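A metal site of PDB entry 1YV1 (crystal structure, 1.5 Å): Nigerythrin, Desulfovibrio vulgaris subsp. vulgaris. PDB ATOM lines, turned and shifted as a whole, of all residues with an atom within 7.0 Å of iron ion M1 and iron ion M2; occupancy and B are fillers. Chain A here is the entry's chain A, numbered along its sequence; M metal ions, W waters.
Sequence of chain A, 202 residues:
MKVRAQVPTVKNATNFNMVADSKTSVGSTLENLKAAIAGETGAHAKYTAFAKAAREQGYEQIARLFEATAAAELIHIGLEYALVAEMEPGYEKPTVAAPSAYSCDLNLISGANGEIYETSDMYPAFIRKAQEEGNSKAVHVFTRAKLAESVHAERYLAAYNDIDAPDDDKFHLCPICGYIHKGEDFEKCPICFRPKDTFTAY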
ATOM      1  N   ALA A  36      -4.796 -11.528  -6.618  1.00  0.00           N
ATOM      2  CA  ALA A  36      -3.410 -11.987  -6.638  1.00  0.00           C
ATOM      3  C   ALA A  36      -2.469 -10.784  -6.654  1.00  0.00           C
ATOM      4  O   ALA A  36      -1.487 -10.744  -5.922  1.00  0.00           O
ATOM      5  CB  ALA A  36      -3.174 -12.882  -7.835  1.00  0.00           C
ATOM      6  N   GLY A  39      -2.222  -9.264  -3.331  1.00  0.00           N
ATOM      7  CA  GLY A  39      -1.384 -10.084  -2.479  1.00  0.00           C
ATOM      8  C   GLY A  39       0.093  -9.943  -2.809  1.00  0.00           C
ATOM      9  O   GLY A  39       0.938  -9.885  -1.916  1.00  0.00           O
ATOM     10  N   GLU A  40       0.392  -9.891  -4.103  1.00  0.00           N
ATOM     11  CA  GLU A  40       1.762  -9.753  -4.575  1.00  0.00           C
ATOM     12  C   GLU A  40       2.326  -8.399  -4.147  1.00  0.00           C
ATOM     13  O   GLU A  40       3.504  -8.287  -3.780  1.00  0.00           O
ATOM     14  CB  GLU A  40       1.846  -9.886  -6.101  1.00  0.00           C
ATOM     15  CG  GLU A  40       1.469 -11.244  -6.640  1.00  0.00           C
ATOM     16  CD  GLU A  40       2.608 -12.239  -6.471  1.00  0.00           C
ATOM     17  OE1 GLU A  40       3.747 -11.796  -6.242  1.00  0.00           O
ATOM     18  OE2 GLU A  40       2.349 -13.452  -6.587  1.00  0.00           O
ATOM     19  N   ALA A  43       3.167  -8.586  -0.633  1.00  0.00           N
ATOM     20  CA  ALA A  43       4.384  -9.366  -0.458  1.00  0.00           C
ATOM     21  C   ALA A  43       5.621  -8.533  -0.776  1.00  0.00           C
ATOM     22  O   ALA A  43       6.616  -8.580  -0.055  1.00  0.00           O
ATOM     23  CB  ALA A  43       4.348 -10.612  -1.353  1.00  0.00           C
ATOM     24  N   TYR A  47       8.530  -7.888   1.900  1.00  0.00           N
ATOM     25  CA  TYR A  47       9.922  -8.270   1.698  1.00  0.00           C
ATOM     26  C   TYR A  47      10.855  -7.076   1.636  1.00  0.00           C
ATOM     27  O   TYR A  47      12.011  -7.176   2.062  1.00  0.00           O
ATOM     28  CB  TYR A  47      10.022  -9.132   0.428  1.00  0.00           C
ATOM     29  CG  TYR A  47       9.238 -10.426   0.542  1.00  0.00           C
ATOM     30  CD1 TYR A  47       8.894 -11.163  -0.596  1.00  0.00           C
ATOM     31  CD2 TYR A  47       8.852 -10.922   1.787  1.00  0.00           C
ATOM     32  CE1 TYR A  47       8.180 -12.353  -0.487  1.00  0.00           C
ATOM     33  CE2 TYR A  47       8.140 -12.119   1.903  1.00  0.00           C
ATOM     34  CZ  TYR A  47       7.807 -12.821   0.763  1.00  0.00           C
ATOM     35  OH  TYR A  47       7.096 -13.995   0.886  1.00  0.00           O
ATOM     36  N   THR A  69      13.619 -11.719  -3.670  1.00  0.00           N
ATOM     37  CA  THR A  69      12.255 -12.238  -3.651  1.00  0.00           C
ATOM     38  C   THR A  69      11.259 -11.103  -3.887  1.00  0.00           C
ATOM     39  O   THR A  69      10.241 -11.307  -4.530  1.00  0.00           O
ATOM     40  CB  THR A  69      11.962 -12.948  -2.324  1.00  0.00           C
ATOM     41  OG1 THR A  69      13.020 -13.880  -2.044  1.00  0.00           O
ATOM     42  CG2 THR A  69      10.643 -13.738  -2.417  1.00  0.00           C
ATOM     43  N   ALA A  72      11.083 -10.686  -7.363  1.00  0.00           N
ATOM     44  CA  ALA A  72      10.344 -11.798  -7.957  1.00  0.00           C
ATOM     45  C   ALA A  72       8.851 -11.509  -7.935  1.00  0.00           C
ATOM     46  O   ALA A  72       8.141 -11.788  -8.903  1.00  0.00           O
ATOM     47  CB  ALA A  72      10.644 -13.086  -7.204  1.00  0.00           C
ATOM     48  N   GLU A  73       8.366 -10.940  -6.832  1.00  0.00           N
ATOM     49  CA  GLU A  73       6.936 -10.647  -6.734  1.00  0.00           C
ATOM     50  C   GLU A  73       6.562  -9.541  -7.713  1.00  0.00           C
ATOM     51  O   GLU A  73       5.427  -9.498  -8.209  1.00  0.00           O
ATOM     52  CB  GLU A  73       6.573 -10.255  -5.295  1.00  0.00           C
ATOM     53  CG  GLU A  73       7.173 -11.161  -4.212  1.00  0.00           C
ATOM     54  CD  GLU A  73       6.964 -12.661  -4.442  1.00  0.00           C
ATOM     55  OE1 GLU A  73       6.370 -13.032  -5.490  1.00  0.00           O
ATOM     56  OE2 GLU A  73       7.356 -13.463  -3.578  1.00  0.00           O
ATOM     57  N   LEU A  74       7.511  -8.646  -8.010  1.00  0.00           N
ATOM     58  CA  LEU A  74       7.237  -7.568  -8.954  1.00  0.00           C
ATOM     59  C   LEU A  74       7.060  -8.165 -10.347  1.00  0.00           C
ATOM     60  O   LEU A  74       6.299  -7.655 -11.165  1.00  0.00           O
ATOM     61  CB  LEU A  74       8.397  -6.566  -8.949  1.00  0.00           C
ATOM     62  CG  LEU A  74       8.156  -5.207  -9.594  1.00  0.00           C
ATOM     63  CD1 LEU A  74       6.911  -4.555  -9.007  1.00  0.00           C
ATOM     64  CD2 LEU A  74       9.376  -4.319  -9.380  1.00  0.00           C
ATOM     65  N   ILE A  75       7.769  -9.264 -10.605  1.00  0.00           N
ATOM     66  CA  ILE A  75       7.674  -9.949 -11.884  1.00  0.00           C
ATOM     67  C   ILE A  75       6.272 -10.562 -11.987  1.00  0.00           C
ATOM     68  O   ILE A  75       5.620 -10.494 -13.033  1.00  0.00           O
ATOM     69  CB  ILE A  75       8.733 -11.078 -11.993  1.00  0.00           C
ATOM     70  CG1 ILE A  75      10.121 -10.451 -12.106  1.00  0.00           C
ATOM     71  CG2 ILE A  75       8.436 -11.969 -13.186  1.00  0.00           C
ATOM     72  CD1 ILE A  75      11.260 -11.461 -12.004  1.00  0.00           C
ATOM     73  N   HIS A  76       5.803 -11.156 -10.893  1.00  0.00           N
ATOM     74  CA  HIS A  76       4.474 -11.757 -10.874  1.00  0.00           C
ATOM     75  C   HIS A  76       3.408 -10.700 -11.098  1.00  0.00           C
ATOM     76  O   HIS A  76       2.444 -10.925 -11.819  1.00  0.00           O
ATOM     77  CB  HIS A  76       4.250 -12.470  -9.533  1.00  0.00           C
ATOM     78  CG  HIS A  76       5.177 -13.626  -9.317  1.00  0.00           C
ATOM     79  ND1 HIS A  76       5.365 -14.209  -8.081  1.00  0.00           N
ATOM     80  CD2 HIS A  76       5.973 -14.294 -10.179  1.00  0.00           C
ATOM     81  CE1 HIS A  76       6.253 -15.186  -8.189  1.00  0.00           C
ATOM     82  NE2 HIS A  76       6.632 -15.253  -9.450  1.00  0.00           N
ATOM     83  N   ILE A  77       3.593  -9.538 -10.480  1.00  0.00           N
ATOM     84  CA  ILE A  77       2.661  -8.421 -10.647  1.00  0.00           C
ATOM     85  C   ILE A  77       2.604  -8.013 -12.121  1.00  0.00           C
ATOM     86  O   ILE A  77       1.528  -7.755 -12.659  1.00  0.00           O
ATOM     87  CB  ILE A  77       3.079  -7.210  -9.797  1.00  0.00           C
ATOM     88  CG1 ILE A  77       2.890  -7.529  -8.307  1.00  0.00           C
ATOM     89  CG2 ILE A  77       2.265  -5.982 -10.183  1.00  0.00           C
ATOM     90  CD1 ILE A  77       3.500  -6.513  -7.366  1.00  0.00           C
ATOM     91  N   GLU A  80       0.560 -10.626 -14.136  1.00  0.00           N
ATOM     92  CA  GLU A  80      -0.862 -10.575 -13.824  1.00  0.00           C
ATOM     93  C   GLU A  80      -1.500  -9.262 -14.270  1.00  0.00           C
ATOM     94  O   GLU A  80      -2.632  -9.245 -14.749  1.00  0.00           O
ATOM     95  CB  GLU A  80      -1.051 -10.803 -12.325  1.00  0.00           C
ATOM     96  CG  GLU A  80      -0.373 -12.102 -11.882  1.00  0.00           C
ATOM     97  CD  GLU A  80      -0.401 -12.340 -10.381  1.00  0.00           C
ATOM     98  OE1 GLU A  80      -0.451 -11.375  -9.601  1.00  0.00           O
ATOM     99  OE2 GLU A  80      -0.341 -13.527  -9.987  1.00  0.00           O
ATOM    100  N   GLY A 111       7.630 -14.973   5.883  1.00  0.00           N
ATOM    101  CA  GLY A 111       7.730 -15.069   4.437  1.00  0.00           C
ATOM    102  C   GLY A 111       7.380 -16.470   3.961  1.00  0.00           C
ATOM    103  O   GLY A 111       6.566 -16.626   3.054  1.00  0.00           O
ATOM    104  N   GLY A 114       3.647 -17.248   4.038  1.00  0.00           N
ATOM    105  CA  GLY A 114       2.870 -16.635   2.973  1.00  0.00           C
ATOM    106  C   GLY A 114       3.072 -17.365   1.656  1.00  0.00           C
ATOM    107  O   GLY A 114       2.124 -17.600   0.908  1.00  0.00           O
ATOM    108  N   GLU A 115       4.323 -17.722   1.377  1.00  0.00           N
ATOM    109  CA  GLU A 115       4.671 -18.443   0.165  1.00  0.00           C
ATOM    110  C   GLU A 115       3.925 -19.775   0.110  1.00  0.00           C
ATOM    111  O   GLU A 115       3.413 -20.169  -0.933  1.00  0.00           O
ATOM    112  CB  GLU A 115       6.175 -18.725   0.118  1.00  0.00           C
ATOM    113  CG  GLU A 115       7.049 -17.490   0.153  1.00  0.00           C
ATOM    114  CD  GLU A 115       6.993 -16.662  -1.124  1.00  0.00           C
ATOM    115  OE1 GLU A 115       6.427 -17.134  -2.133  1.00  0.00           O
ATOM    116  OE2 GLU A 115       7.514 -15.519  -1.123  1.00  0.00           O
ATOM    117  N   GLU A 118       0.259 -19.277  -0.722  1.00  0.00           N
ATOM    118  CA  GLU A 118       0.070 -18.976  -2.131  1.00  0.00           C
ATOM    119  C   GLU A 118       0.272 -20.178  -3.047  1.00  0.00           C
ATOM    120  O   GLU A 118      -0.482 -20.364  -4.001  1.00  0.00           O
ATOM    121  CB  GLU A 118       1.009 -17.853  -2.544  1.00  0.00           C
ATOM    122  CG  GLU A 118       0.759 -16.549  -1.811  1.00  0.00           C
ATOM    123  CD  GLU A 118       1.991 -15.660  -1.751  1.00  0.00           C
ATOM    124  OE1 GLU A 118       1.906 -14.549  -1.176  1.00  0.00           O
ATOM    125  OE2 GLU A 118       3.046 -16.089  -2.269  1.00  0.00           O
ATOM    126  N   TYR A 123      -3.020 -19.833  -5.294  1.00  0.00           N
ATOM    127  CA  TYR A 123      -2.803 -20.052  -6.723  1.00  0.00           C
ATOM    128  C   TYR A 123      -3.452 -21.317  -7.290  1.00  0.00           C
ATOM    129  O   TYR A 123      -4.005 -21.284  -8.374  1.00  0.00           O
ATOM    130  CB  TYR A 123      -1.319 -19.938  -7.065  1.00  0.00           C
ATOM    131  CG  TYR A 123      -0.880 -18.486  -7.179  1.00  0.00           C
ATOM    132  CD1 TYR A 123       0.210 -17.993  -6.465  1.00  0.00           C
ATOM    133  CD2 TYR A 123      -1.584 -17.590  -8.000  1.00  0.00           C
ATOM    134  CE1 TYR A 123       0.588 -16.644  -6.562  1.00  0.00           C
ATOM    135  CE2 TYR A 123      -1.223 -16.259  -8.094  1.00  0.00           C
ATOM    136  CZ  TYR A 123      -0.141 -15.786  -7.381  1.00  0.00           C
ATOM    137  OH  TYR A 123       0.216 -14.462  -7.478  1.00  0.00           O
ATOM    138  N   ALA A 145       3.583 -18.225 -11.233  1.00  0.00           N
ATOM    139  CA  ALA A 145       3.685 -17.623  -9.918  1.00  0.00           C
ATOM    140  C   ALA A 145       3.678 -18.729  -8.856  1.00  0.00           C
ATOM    141  O   ALA A 145       4.517 -18.745  -7.970  1.00  0.00           O
ATOM    142  CB  ALA A 145       2.527 -16.660  -9.684  1.00  0.00           C
ATOM    143  N   LYS A 146       2.722 -19.648  -8.974  1.00  0.00           N
ATOM    144  CA  LYS A 146       2.583 -20.773  -8.044  1.00  0.00           C
ATOM    145  C   LYS A 146       3.888 -21.549  -7.870  1.00  0.00           C
ATOM    146  O   LYS A 146       4.299 -21.841  -6.752  1.00  0.00           O
ATOM    147  CB  LYS A 146       1.470 -21.705  -8.526  1.00  0.00           C
ATOM    148  CG  LYS A 146       1.249 -22.986  -7.716  1.00  0.00           C
ATOM    149  CD  LYS A 146       2.156 -24.124  -8.201  1.00  0.00           C
ATOM    150  CE  LYS A 146       1.793 -25.465  -7.555  1.00  0.00           C
ATOM    151  NZ  LYS A 146       2.100 -25.527  -6.092  1.00  0.00           N
ATOM    152  N   ALA A 148       6.933 -20.543  -8.543  1.00  0.00           N
ATOM    153  CA  ALA A 148       7.974 -19.709  -7.969  1.00  0.00           C
ATOM    154  C   ALA A 148       7.816 -19.556  -6.454  1.00  0.00           C
ATOM    155  O   ALA A 148       8.805 -19.563  -5.723  1.00  0.00           O
ATOM    156  CB  ALA A 148       7.965 -18.334  -8.629  1.00  0.00           C
ATOM    157  N   GLU A 149       6.577 -19.462  -5.980  1.00  0.00           N
ATOM    158  CA  GLU A 149       6.345 -19.284  -4.554  1.00  0.00           C
ATOM    159  C   GLU A 149       6.840 -20.466  -3.711  1.00  0.00           C
ATOM    160  O   GLU A 149       7.380 -20.259  -2.621  1.00  0.00           O
ATOM    161  CB  GLU A 149       4.848 -19.059  -4.257  1.00  0.00           C
ATOM    162  CG  GLU A 149       4.157 -18.129  -5.245  1.00  0.00           C
ATOM    163  CD  GLU A 149       4.695 -16.711  -5.287  1.00  0.00           C
ATOM    164  OE1 GLU A 149       5.855 -16.497  -4.906  1.00  0.00           O
ATOM    165  OE2 GLU A 149       3.950 -15.809  -5.719  1.00  0.00           O
ATOM    166  N   SER A 150       6.672 -21.697  -4.190  1.00  0.00           N
ATOM    167  CA  SER A 150       7.160 -22.824  -3.407  1.00  0.00           C
ATOM    168  C   SER A 150       8.680 -22.821  -3.352  1.00  0.00           C
ATOM    169  O   SER A 150       9.273 -23.261  -2.372  1.00  0.00           O
ATOM    170  CB  SER A 150       6.618 -24.156  -3.946  1.00  0.00           C
ATOM    171  OG  SER A 150       6.968 -24.375  -5.287  1.00  0.00           O
ATOM    172  N   HIS A 152      10.451 -20.029  -3.341  1.00  0.00           N
ATOM    173  CA  HIS A 152      10.718 -18.969  -2.375  1.00  0.00           C
ATOM    174  C   HIS A 152      10.623 -19.512  -0.948  1.00  0.00           C
ATOM    175  O   HIS A 152      11.450 -19.185  -0.090  1.00  0.00           O
ATOM    176  CB  HIS A 152       9.746 -17.838  -2.515  1.00  0.00           C
ATOM    177  CG  HIS A 152       9.812 -17.125  -3.867  1.00  0.00           C
ATOM    178  ND1 HIS A 152       8.845 -16.252  -4.299  1.00  0.00           N
ATOM    179  CD2 HIS A 152      10.747 -17.181  -4.841  1.00  0.00           C
ATOM    180  CE1 HIS A 152       9.185 -15.790  -5.501  1.00  0.00           C
ATOM    181  NE2 HIS A 152      10.334 -16.347  -5.848  1.00  0.00           N
ATOM    182  N   ALA A 153       9.616 -20.333  -0.702  1.00  0.00           N
ATOM    183  CA  ALA A 153       9.421 -20.918   0.616  1.00  0.00           C
ATOM    184  C   ALA A 153      10.643 -21.725   1.039  1.00  0.00           C
ATOM    185  O   ALA A 153      11.127 -21.589   2.157  1.00  0.00           O
ATOM    186  CB  ALA A 153       8.182 -21.812   0.623  1.00  0.00           C
ATOM    187  N   TYR A 156      13.602 -19.513   1.873  1.00  0.00           N
ATOM    188  CA  TYR A 156      13.448 -18.863   3.171  1.00  0.00           C
ATOM    189  C   TYR A 156      13.767 -19.832   4.315  1.00  0.00           C
ATOM    190  O   TYR A 156      14.399 -19.452   5.302  1.00  0.00           O
ATOM    191  CB  TYR A 156      12.027 -18.297   3.309  1.00  0.00           C
ATOM    192  CG  TYR A 156      11.810 -16.984   2.575  1.00  0.00           C
ATOM    193  CD1 TYR A 156      10.537 -16.631   2.121  1.00  0.00           C
ATOM    194  CD2 TYR A 156      12.855 -16.085   2.383  1.00  0.00           C
ATOM    195  CE1 TYR A 156      10.317 -15.396   1.498  1.00  0.00           C
ATOM    196  CE2 TYR A 156      12.640 -14.843   1.764  1.00  0.00           C
ATOM    197  CZ  TYR A 156      11.367 -14.509   1.321  1.00  0.00           C
ATOM    198  OH  TYR A 156      11.158 -13.277   0.734  1.00  0.00           O
ATOM    199  N   CYS A 177       9.917 -15.781 -14.632  1.00  0.00           N
ATOM    200  CA  CYS A 177       8.986 -16.364 -13.677  1.00  0.00           C
ATOM    201  C   CYS A 177       9.242 -16.076 -12.209  1.00  0.00           C
ATOM    202  O   CYS A 177       8.414 -16.409 -11.362  1.00  0.00           O
ATOM    203  CB  CYS A 177       8.948 -17.879 -13.885  1.00  0.00           C
ATOM    204  SG  CYS A 177      10.466 -18.709 -13.397  1.00  0.00           S
ATOM    205  N   GLY A 178      10.382 -15.480 -11.889  1.00  0.00           N
ATOM    206  CA  GLY A 178      10.654 -15.189 -10.493  1.00  0.00           C
ATOM    207  C   GLY A 178      11.369 -16.287  -9.739  1.00  0.00           C
ATOM    208  O   GLY A 178      11.498 -16.226  -8.517  1.00  0.00           O
HETATM  209 FE    FE M   1       6.931 -15.441  -3.430  1.00  0.00          FE
HETATM  210 FE    FE M   2       4.565 -13.894  -6.113  1.00  0.00          FE
HETATM  211  O   HOH W   1       5.164 -14.571  -2.330  1.00  0.00           O
HETATM  212  O   HOH W   2       3.609 -13.591  -3.975  1.00  0.00           O
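Iron ion M2 is bound by the side-chain carboxylate (OE2) of Glu 149 (2.0 Å), the side-chain carboxylate (OE1) of Glu 73 (2.1 Å), a ring nitrogen (ND1) of His 76 (2.1 Å), the side-chain carboxylate (OE1) of Glu 40 (2.3 Å), the side-chain carboxylate (OE2) of Glu 40 (2.3 Å) and water W2 (2.4 Å).
Four residues have an atom within 4 Å of iron ion M1: Glu 73, Glu 115, Glu 149 and His 152.
The nearest printed residue that does not touch iron ion M1 is Glu 118 (4.1 Å).
The backbone carbonyl oxygen (O) of Cys 177 is in hydrogen-bond range of a ring nitrogen (NE2) of His 76.
The side-chain carboxylate (OE2) of Glu 115 sits close to the side-chain hydroxyl (OH) of Tyr 47, at 2.6 Å.
The backbone carbonyl oxygen (O) of Gly 178 lies within hydrogen-bond range of a ring nitrogen (NE2) of His 152 (2.9 Å).
The side-chain hydroxyl (OH) of Tyr 123 lies close to the side-chain carboxylate (OE2) of Glu 40.
OE2 of Glu 73 is bound to iron ion M1 (2.0 Å).
OE1 of Glu 149 binds iron ion M1, 2.1 Å away.
Iron ion M1 is bound by the side-chain carboxylate (OE1) of Glu 115, 2.2 Å away.
A ring nitrogen (ND1) of His 152 is bound to iron ion M1.
Water W1 is bound to iron ion M1 (2.3 Å).
Iron ion M1 is bound by OE2 of Glu 115, at 2.4 Å.
Iron ion M1 has six donor atoms within binding distance.
Within 4 Å of iron ion M2: Glu 40, Glu 73, His 76 and Glu 149.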
